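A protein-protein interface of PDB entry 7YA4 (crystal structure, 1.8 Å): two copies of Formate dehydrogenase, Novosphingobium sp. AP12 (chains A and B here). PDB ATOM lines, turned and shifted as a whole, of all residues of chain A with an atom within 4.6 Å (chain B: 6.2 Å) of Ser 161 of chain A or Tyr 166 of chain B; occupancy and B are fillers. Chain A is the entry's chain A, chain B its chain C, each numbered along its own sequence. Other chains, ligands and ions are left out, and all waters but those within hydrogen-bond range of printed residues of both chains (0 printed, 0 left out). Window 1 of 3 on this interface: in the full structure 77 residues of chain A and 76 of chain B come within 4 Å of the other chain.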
ATOM      1  N   MET A 157     -14.793   6.405   2.922  1.00  0.00           N
ATOM      2  CA  MET A 157     -14.232   7.744   2.866  1.00  0.00           C
ATOM      3  C   MET A 157     -13.221   7.871   1.720  1.00  0.00           C
ATOM      4  O   MET A 157     -13.268   8.858   0.959  1.00  0.00           O
ATOM      5  CB  MET A 157     -13.574   8.069   4.222  1.00  0.00           C
ATOM      6  CG  MET A 157     -12.821   9.370   4.274  1.00  0.00           C
ATOM      7  SD  MET A 157     -11.917   9.484   5.849  1.00  0.00           S
ATOM      8  CE  MET A 157     -10.523   8.441   5.504  1.00  0.00           C
ATOM      9  N   MET A 158     -12.346   6.862   1.563  1.00  0.00           N
ATOM     10  CA  MET A 158     -11.317   6.883   0.546  1.00  0.00           C
ATOM     11  C   MET A 158     -11.894   6.643  -0.855  1.00  0.00           C
ATOM     12  O   MET A 158     -11.453   7.289  -1.803  1.00  0.00           O
ATOM     13  CB  MET A 158     -10.247   5.833   0.864  1.00  0.00           C
ATOM     14  CG  MET A 158      -9.283   6.311   1.912  1.00  0.00           C
ATOM     15  SD  MET A 158      -8.091   5.051   2.361  1.00  0.00           S
ATOM     16  CE  MET A 158      -6.931   6.086   3.288  1.00  0.00           C
ATOM     17  N   ILE A 159     -12.924   5.822  -0.969  1.00  0.00           N
ATOM     18  CA  ILE A 159     -13.589   5.628  -2.271  1.00  0.00           C
ATOM     19  C   ILE A 159     -14.168   6.968  -2.751  1.00  0.00           C
ATOM     20  O   ILE A 159     -13.881   7.430  -3.853  1.00  0.00           O
ATOM     21  CB  ILE A 159     -14.696   4.545  -2.200  1.00  0.00           C
ATOM     22  CG1 ILE A 159     -14.119   3.156  -1.966  1.00  0.00           C
ATOM     23  CG2 ILE A 159     -15.547   4.559  -3.465  1.00  0.00           C
ATOM     24  CD1 ILE A 159     -15.170   2.063  -1.728  1.00  0.00           C
ATOM     25  N   LEU A 160     -14.909   7.660  -1.873  1.00  0.00           N
ATOM     26  CA  LEU A 160     -15.543   8.928  -2.229  1.00  0.00           C
ATOM     27  C   LEU A 160     -14.458   9.973  -2.503  1.00  0.00           C
ATOM     28  O   LEU A 160     -14.602  10.751  -3.447  1.00  0.00           O
ATOM     29  CB  LEU A 160     -16.459   9.446  -1.115  1.00  0.00           C
ATOM     30  CG  LEU A 160     -17.658   8.588  -0.734  1.00  0.00           C
ATOM     31  CD1 LEU A 160     -18.422   9.161   0.450  1.00  0.00           C
ATOM     32  CD2 LEU A 160     -18.578   8.392  -1.914  1.00  0.00           C
ATOM     33  N   SER A 161     -13.381  10.008  -1.698  1.00  0.00           N
ATOM     34  CA  SER A 161     -12.359  11.029  -1.919  1.00  0.00           C
ATOM     35  C   SER A 161     -11.663  10.877  -3.276  1.00  0.00           C
ATOM     36  O   SER A 161     -11.385  11.884  -3.935  1.00  0.00           O
ATOM     37  CB  SER A 161     -11.379  11.085  -0.770  1.00  0.00           C
ATOM     38  OG  SER A 161     -12.104  11.397   0.448  1.00  0.00           O
ATOM     39  N   LEU A 162     -11.285   9.659  -3.648  1.00  0.00           N
ATOM     40  CA  LEU A 162     -10.683   9.361  -4.957  1.00  0.00           C
ATOM     41  C   LEU A 162     -11.601   9.782  -6.106  1.00  0.00           C
ATOM     42  O   LEU A 162     -11.183  10.509  -7.018  1.00  0.00           O
ATOM     43  CB  LEU A 162     -10.338   7.876  -5.090  1.00  0.00           C
ATOM     44  CG  LEU A 162      -9.116   7.398  -4.315  1.00  0.00           C
ATOM     45  CD1 LEU A 162      -8.865   5.927  -4.584  1.00  0.00           C
ATOM     46  CD2 LEU A 162      -7.880   8.207  -4.655  1.00  0.00           C
ATOM     47  N   VAL A 163     -12.842   9.303  -6.051  1.00  0.00           N
ATOM     48  CA  VAL A 163     -13.779   9.465  -7.140  1.00  0.00           C
ATOM     49  C   VAL A 163     -14.116  10.947  -7.323  1.00  0.00           C
ATOM     50  O   VAL A 163     -14.171  11.406  -8.447  1.00  0.00           O
ATOM     51  CB  VAL A 163     -15.005   8.563  -6.878  1.00  0.00           C
ATOM     52  CG1 VAL A 163     -16.171   8.871  -7.799  1.00  0.00           C
ATOM     53  CG2 VAL A 163     -14.652   7.091  -6.960  1.00  0.00           C
ATOM     54  N   ARG A 164     -14.272  11.707  -6.212  1.00  0.00           N
ATOM     55  CA  ARG A 164     -14.752  13.090  -6.258  1.00  0.00           C
ATOM     56  C   ARG A 164     -13.573  14.066  -6.413  1.00  0.00           C
ATOM     57  O   ARG A 164     -13.813  15.254  -6.548  1.00  0.00           O
ATOM     58  CB  ARG A 164     -15.570  13.460  -5.015  1.00  0.00           C
ATOM     59  CG  ARG A 164     -16.854  12.667  -4.828  1.00  0.00           C
ATOM     60  CD  ARG A 164     -17.816  13.362  -3.886  1.00  0.00           C
ATOM     61  NE  ARG A 164     -18.340  14.609  -4.447  1.00  0.00           N
ATOM     62  CZ  ARG A 164     -19.161  14.677  -5.496  1.00  0.00           C
ATOM     63  NH1 ARG A 164     -19.843  13.594  -5.870  1.00  0.00           N
ATOM     64  NH2 ARG A 164     -19.362  15.867  -6.067  1.00  0.00           N
ATOM     65  N   ASN A 165     -12.325  13.570  -6.315  1.00  0.00           N
ATOM     66  CA  ASN A 165     -11.129  14.398  -6.444  1.00  0.00           C
ATOM     67  C   ASN A 165     -10.976  15.362  -5.251  1.00  0.00           C
ATOM     68  O   ASN A 165     -10.560  16.519  -5.376  1.00  0.00           O
ATOM     69  CB  ASN A 165     -11.097  15.151  -7.765  1.00  0.00           C
ATOM     70  CG  ASN A 165      -9.697  15.491  -8.231  1.00  0.00           C
ATOM     71  OD1 ASN A 165      -8.796  14.652  -8.064  1.00  0.00           O
ATOM     72  ND2 ASN A 165      -9.512  16.684  -8.809  1.00  0.00           N
ATOM     73  N   TYR A 166     -11.278  14.860  -4.068  1.00  0.00           N
ATOM     74  CA  TYR A 166     -11.275  15.684  -2.867  1.00  0.00           C
ATOM     75  C   TYR A 166      -9.911  16.291  -2.553  1.00  0.00           C
ATOM     76  O   TYR A 166      -9.813  17.483  -2.240  1.00  0.00           O
ATOM     77  CB  TYR A 166     -11.749  14.810  -1.711  1.00  0.00           C
ATOM     78  CG  TYR A 166     -11.953  15.527  -0.400  1.00  0.00           C
ATOM     79  CD1 TYR A 166     -12.117  16.899  -0.310  1.00  0.00           C
ATOM     80  CD2 TYR A 166     -12.132  14.789   0.755  1.00  0.00           C
ATOM     81  CE1 TYR A 166     -12.385  17.536   0.908  1.00  0.00           C
ATOM     82  CE2 TYR A 166     -12.414  15.402   1.972  1.00  0.00           C
ATOM     83  CZ  TYR A 166     -12.546  16.775   2.056  1.00  0.00           C
ATOM     84  OH  TYR A 166     -12.848  17.387   3.275  1.00  0.00           O
ATOM     85  N   ILE A 167      -8.857  15.456  -2.477  1.00  0.00           N
ATOM     86  CA  ILE A 167      -7.591  15.921  -1.917  1.00  0.00           C
ATOM     87  C   ILE A 167      -7.001  17.021  -2.809  1.00  0.00           C
ATOM     88  O   ILE A 167      -6.653  18.086  -2.305  1.00  0.00           O
ATOM     89  CB  ILE A 167      -6.620  14.750  -1.663  1.00  0.00           C
ATOM     90  CG1 ILE A 167      -7.071  13.958  -0.430  1.00  0.00           C
ATOM     91  CG2 ILE A 167      -5.184  15.256  -1.544  1.00  0.00           C
ATOM     92  CD1 ILE A 167      -6.391  12.633  -0.295  1.00  0.00           C
ATOM     93  N   GLY A 329      -4.567   8.789  -2.393  1.00  0.00           N
ATOM     94  CA  GLY A 329      -5.252   9.271  -1.208  1.00  0.00           C
ATOM     95  C   GLY A 329      -4.820   8.537   0.048  1.00  0.00           C
ATOM     96  O   GLY A 329      -5.660   8.263   0.925  1.00  0.00           O
ATOM     97  N   MET A 330      -3.500   8.281   0.129  1.00  0.00           N
ATOM     98  CA  MET A 330      -2.921   7.495   1.206  1.00  0.00           C
ATOM     99  C   MET A 330      -3.050   8.166   2.588  1.00  0.00           C
ATOM    100  O   MET A 330      -3.051   9.397   2.710  1.00  0.00           O
ATOM    101  CB  MET A 330      -1.426   7.226   0.978  1.00  0.00           C
ATOM    102  CG  MET A 330      -1.137   6.465  -0.321  1.00  0.00           C
ATOM    103  SD  MET A 330      -1.899   4.844  -0.470  1.00  0.00           S
ATOM    104  CE  MET A 330      -1.110   3.866   0.797  1.00  0.00           C
ATOM    105  N   THR A 331      -3.157   7.318   3.616  1.00  0.00           N
ATOM    106  CA  THR A 331      -2.795   7.733   4.969  1.00  0.00           C
ATOM    107  C   THR A 331      -1.741   6.767   5.505  1.00  0.00           C
ATOM    108  O   THR A 331      -1.602   5.661   4.971  1.00  0.00           O
ATOM    109  CB  THR A 331      -3.987   7.797   5.924  1.00  0.00           C
ATOM    110  OG1 THR A 331      -4.544   6.493   6.101  1.00  0.00           O
ATOM    111  CG2 THR A 331      -5.056   8.766   5.498  1.00  0.00           C
ATOM    112  N   MET B 157     -18.764  12.526   2.327  1.00  0.00           N
ATOM    113  CA  MET B 157     -17.314  12.430   2.235  1.00  0.00           C
ATOM    114  C   MET B 157     -16.667  13.325   3.310  1.00  0.00           C
ATOM    115  O   MET B 157     -15.723  12.928   3.990  1.00  0.00           O
ATOM    116  CB  MET B 157     -16.891  12.885   0.841  1.00  0.00           C
ATOM    117  CG  MET B 157     -15.419  12.809   0.579  1.00  0.00           C
ATOM    118  SD  MET B 157     -15.073  13.511  -1.060  1.00  0.00           S
ATOM    119  CE  MET B 157     -15.309  15.247  -0.727  1.00  0.00           C
ATOM    120  N   LEU B 160     -17.045  12.157   7.033  1.00  0.00           N
ATOM    121  CA  LEU B 160     -16.152  11.065   7.390  1.00  0.00           C
ATOM    122  C   LEU B 160     -14.727  11.588   7.528  1.00  0.00           C
ATOM    123  O   LEU B 160     -14.026  11.208   8.462  1.00  0.00           O
ATOM    124  CB  LEU B 160     -16.195   9.946   6.347  1.00  0.00           C
ATOM    125  CG  LEU B 160     -17.525   9.235   6.194  1.00  0.00           C
ATOM    126  CD1 LEU B 160     -17.443   8.214   5.061  1.00  0.00           C
ATOM    127  CD2 LEU B 160     -17.948   8.584   7.495  1.00  0.00           C
ATOM    128  N   SER B 161     -14.305  12.451   6.599  1.00  0.00           N
ATOM    129  CA  SER B 161     -12.966  13.020   6.614  1.00  0.00           C
ATOM    130  C   SER B 161     -12.672  13.828   7.892  1.00  0.00           C
ATOM    131  O   SER B 161     -11.560  13.722   8.414  1.00  0.00           O
ATOM    132  CB  SER B 161     -12.704  13.857   5.390  1.00  0.00           C
ATOM    133  OG  SER B 161     -12.892  13.043   4.206  1.00  0.00           O
ATOM    134  N   LEU B 162     -13.635  14.618   8.367  1.00  0.00           N
ATOM    135  CA  LEU B 162     -13.446  15.395   9.587  1.00  0.00           C
ATOM    136  C   LEU B 162     -13.341  14.478  10.801  1.00  0.00           C
ATOM    137  O   LEU B 162     -12.434  14.613  11.611  1.00  0.00           O
ATOM    138  CB  LEU B 162     -14.610  16.372   9.779  1.00  0.00           C
ATOM    139  CG  LEU B 162     -14.695  17.576   8.838  1.00  0.00           C
ATOM    140  CD1 LEU B 162     -15.831  18.450   9.289  1.00  0.00           C
ATOM    141  CD2 LEU B 162     -13.411  18.369   8.808  1.00  0.00           C
ATOM    142  N   VAL B 163     -14.263  13.531  10.923  1.00  0.00           N
ATOM    143  CA  VAL B 163     -14.349  12.724  12.138  1.00  0.00           C
ATOM    144  C   VAL B 163     -13.114  11.824  12.288  1.00  0.00           C
ATOM    145  O   VAL B 163     -12.543  11.698  13.361  1.00  0.00           O
ATOM    146  CB  VAL B 163     -15.671  11.940  12.154  1.00  0.00           C
ATOM    147  CG1 VAL B 163     -15.693  10.931  13.277  1.00  0.00           C
ATOM    148  CG2 VAL B 163     -16.872  12.861  12.258  1.00  0.00           C
ATOM    149  N   ARG B 164     -12.648  11.269  11.161  1.00  0.00           N
ATOM    150  CA  ARG B 164     -11.533  10.334  11.099  1.00  0.00           C
ATOM    151  C   ARG B 164     -10.181  11.043  10.989  1.00  0.00           C
ATOM    152  O   ARG B 164      -9.169  10.384  11.111  1.00  0.00           O
ATOM    153  CB  ARG B 164     -11.759   9.402   9.911  1.00  0.00           C
ATOM    154  CG  ARG B 164     -13.000   8.528  10.097  1.00  0.00           C
ATOM    155  CD  ARG B 164     -13.012   7.331   9.143  1.00  0.00           C
ATOM    156  NE  ARG B 164     -12.033   6.379   9.608  1.00  0.00           N
ATOM    157  CZ  ARG B 164     -12.131   5.605  10.679  1.00  0.00           C
ATOM    158  NH1 ARG B 164     -13.300   5.384  11.268  1.00  0.00           N
ATOM    159  NH2 ARG B 164     -11.041   5.012  11.130  1.00  0.00           N
ATOM    160  N   ASN B 165     -10.177  12.359  10.776  1.00  0.00           N
ATOM    161  CA  ASN B 165      -8.928  13.128  10.693  1.00  0.00           C
ATOM    162  C   ASN B 165      -8.109  12.722   9.467  1.00  0.00           C
ATOM    163  O   ASN B 165      -6.890  12.641   9.532  1.00  0.00           O
ATOM    164  CB  ASN B 165      -8.071  12.997  11.962  1.00  0.00           C
ATOM    165  CG  ASN B 165      -7.151  14.185  12.216  1.00  0.00           C
ATOM    166  OD1 ASN B 165      -7.564  15.326  12.037  1.00  0.00           O
ATOM    167  ND2 ASN B 165      -5.934  13.933  12.681  1.00  0.00           N
ATOM    168  N   TYR B 166      -8.778  12.596   8.323  1.00  0.00           N
ATOM    169  CA  TYR B 166      -8.167  12.109   7.108  1.00  0.00           C
ATOM    170  C   TYR B 166      -7.113  13.087   6.603  1.00  0.00           C
ATOM    171  O   TYR B 166      -6.013  12.676   6.270  1.00  0.00           O
ATOM    172  CB  TYR B 166      -9.245  12.003   6.023  1.00  0.00           C
ATOM    173  CG  TYR B 166      -8.823  11.478   4.672  1.00  0.00           C
ATOM    174  CD1 TYR B 166      -7.714  10.667   4.506  1.00  0.00           C
ATOM    175  CD2 TYR B 166      -9.659  11.635   3.586  1.00  0.00           C
ATOM    176  CE1 TYR B 166      -7.406  10.120   3.258  1.00  0.00           C
ATOM    177  CE2 TYR B 166      -9.372  11.075   2.350  1.00  0.00           C
ATOM    178  CZ  TYR B 166      -8.247  10.289   2.195  1.00  0.00           C
ATOM    179  OH  TYR B 166      -7.912   9.718   0.982  1.00  0.00           O
ATOM    180  N   ILE B 167      -7.447  14.377   6.492  1.00  0.00           N
ATOM    181  CA  ILE B 167      -6.597  15.269   5.699  1.00  0.00           C
ATOM    182  C   ILE B 167      -5.233  15.463   6.349  1.00  0.00           C
ATOM    183  O   ILE B 167      -4.201  15.366   5.671  1.00  0.00           O
ATOM    184  CB  ILE B 167      -7.291  16.591   5.296  1.00  0.00           C
ATOM    185  CG1 ILE B 167      -8.361  16.348   4.234  1.00  0.00           C
ATOM    186  CG2 ILE B 167      -6.269  17.614   4.778  1.00  0.00           C
ATOM    187  CD1 ILE B 167      -9.401  17.450   4.125  1.00  0.00           C
ATOM    188  N   PRO B 168      -5.156  15.778   7.668  1.00  0.00           N
ATOM    189  CA  PRO B 168      -3.863  15.857   8.336  1.00  0.00           C
ATOM    190  C   PRO B 168      -3.066  14.567   8.196  1.00  0.00           C
ATOM    191  O   PRO B 168      -1.865  14.631   7.939  1.00  0.00           O
ATOM    192  CB  PRO B 168      -4.208  16.162   9.805  1.00  0.00           C
ATOM    193  CG  PRO B 168      -5.536  16.864   9.682  1.00  0.00           C
ATOM    194  CD  PRO B 168      -6.269  16.100   8.563  1.00  0.00           C
ATOM    195  N   ALA B 169      -3.715  13.402   8.304  1.00  0.00           N
ATOM    196  CA  ALA B 169      -3.002  12.136   8.133  1.00  0.00           C
ATOM    197  C   ALA B 169      -2.433  11.999   6.709  1.00  0.00           C
ATOM    198  O   ALA B 169      -1.322  11.459   6.520  1.00  0.00           O
ATOM    199  CB  ALA B 169      -3.936  10.997   8.483  1.00  0.00           C
ATOM    200  N   HIS B 170      -3.206  12.457   5.699  1.00  0.00           N
ATOM    201  CA  HIS B 170      -2.722  12.393   4.339  1.00  0.00           C
ATOM    202  C   HIS B 170      -1.519  13.311   4.160  1.00  0.00           C
ATOM    203  O   HIS B 170      -0.602  12.920   3.455  1.00  0.00           O
ATOM    204  CB  HIS B 170      -3.767  12.712   3.265  1.00  0.00           C
ATOM    205  CG  HIS B 170      -3.176  12.762   1.888  1.00  0.00           C
ATOM    206  ND1 HIS B 170      -2.911  11.646   1.109  1.00  0.00           N
ATOM    207  CD2 HIS B 170      -2.833  13.862   1.131  1.00  0.00           C
ATOM    208  CE1 HIS B 170      -2.388  12.040  -0.053  1.00  0.00           C
ATOM    209  NE2 HIS B 170      -2.358  13.412  -0.079  1.00  0.00           N
ATOM    210  N   GLU B 171      -1.491  14.472   4.846  1.00  0.00           N
ATOM    211  CA  GLU B 171      -0.326  15.355   4.806  1.00  0.00           C
ATOM    212  C   GLU B 171       0.904  14.636   5.392  1.00  0.00           C
ATOM    213  O   GLU B 171       1.989  14.753   4.859  1.00  0.00           O
ATOM    214  CB  GLU B 171      -0.664  16.670   5.497  1.00  0.00           C
ATOM    215  CG  GLU B 171      -1.723  17.471   4.733  1.00  0.00           C
ATOM    216  CD  GLU B 171      -2.310  18.681   5.433  1.00  0.00           C
ATOM    217  OE1 GLU B 171      -2.030  18.847   6.630  1.00  0.00           O
ATOM    218  OE2 GLU B 171      -3.098  19.422   4.803  1.00  0.00           O
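OH of Tyr 166 of chain B lies within hydrogen-bond range of O of Gly 329 of chain A, at 2.7 Å.
ND1 of His 170 of chain B sits at hydrogen-bond distance from O of Met 330 of chain A, at 2.8 Å.
The side-chain sulfur (SD) of Met 157 of chain A lies close to the backbone carbonyl oxygen (O) of Leu 160 of chain B (3.8 Å).
O of Leu 160 of chain A sits close to SD of Met 157 of chain B, at 3.7 Å.
O of Met 157 of chain A is in hydrogen-bond range of OG of Ser 161 of chain A (2.8 Å).
The backbone carbonyl oxygen (O) of Ser 161 of chain A lies within hydrogen-bond range of the backbone NH (N) of Tyr 166 of chain A (3.0 Å).
The backbone carbonyl oxygen (O) of Met 157 of chain B is in hydrogen-bond range of the side-chain hydroxyl (OG) of Ser 161 of chain B (2.8 Å).
N of Tyr 166 of chain B sits at hydrogen-bond distance from O of Ser 161 of chain B (3.0 Å).
Met 157 of chain A touches Ser 161 of chain B.
Tyr 166 of chain B touches Met 157 of chain A.
Tyr 166 of chain B touches Met 158 of chain A.
Tyr 166 of chain B touches Ser 161 of chain A.
Tyr 166 of chain A touches Met 157 of chain B (CG to CE, 3.4 Å).
Tyr 166 of chain A touches Ser 161 of chain B (CE2 to OG, 3.3 Å).
Tyr 166 of chain A touches Ile 167 of chain B.
Ile 167 of chain A touches His 170 of chain B.
Gly 329 of chain A touches His 170 of chain B.
Tyr 166 of chain B touches Thr 331 of chain A.
Of the printed residues of chain B, Met 158 of chain A touches Tyr 166.
Ser 161 of chain A touches just these residues of chain B: Met 157 and Tyr 166.
Of the printed residues of chain B, Arg 164 of chain A touches Met 157.
Asn 165 of chain A touches none of the printed residues of chain B.
Of the printed residues of chain A, Ser 161 of chain B touches Met 157 and Tyr 166.
Arg 164 of chain B touches none of the printed residues of chain A.
Tyr 166 of chain B touches six residues of chain A.
Printed residues of chain A within 4 Å of Ile 167 of chain B: Tyr 166 (3.6 Å).
The nearest residue of chain B that does not touch Ser 161 of chain A is Ser 161 of chain B (4.2 Å).
The nearest printed residue of chain B that does not touch Ile 167 of chain A is Ile 167 of chain B (5.4 Å).
Of the 14 printed residues of chain A, 10 touch a printed residue of chain B.
Printed residues of chain A that touch a printed residue of chain B: Met 157, Met 158, Leu 160, Ser 161, Arg 164, Tyr 166, Ile 167, Gly 329, Met 330 and Thr 331.
Hydrophobic or aromatic side chains of chain A within 4 Å of the printed part of chain B: Met 157, Met 158, Leu 160, Tyr 166 and Ile 167.
Of the 13 printed residues of chain B, 7 touch a printed residue of chain A.
Among the printed residues, 18 pairs touch across the chains.
Among the printed residues, no Asp or Glu carboxylate lies within 4 Å of a Lys or Arg side-chain nitrogen of the other chain.
Met 157 of chain A touches Tyr 166 of chain B, and with the chains exchanged Tyr 166 of chain A touches Met 157 of chain B.
Ser 161 of chain A touches Tyr 166 of chain B, and with the chains exchanged Tyr 166 of chain A touches Ser 161 of chain B.
Arg 164 of chain A touches Met 157 of chain B, but with the chains exchanged Met 157 of chain A does not touch Arg 164 of chain B (4.1 Å).
Tyr 166 of chain A touches Ile 167 of chain B, and with the chains exchanged Ile 167 of chain A touches Tyr 166 of chain B.
Of the 18 pairs that touch across the chains among the printed residues, 10 have their exchanged pair printed and touching as well.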
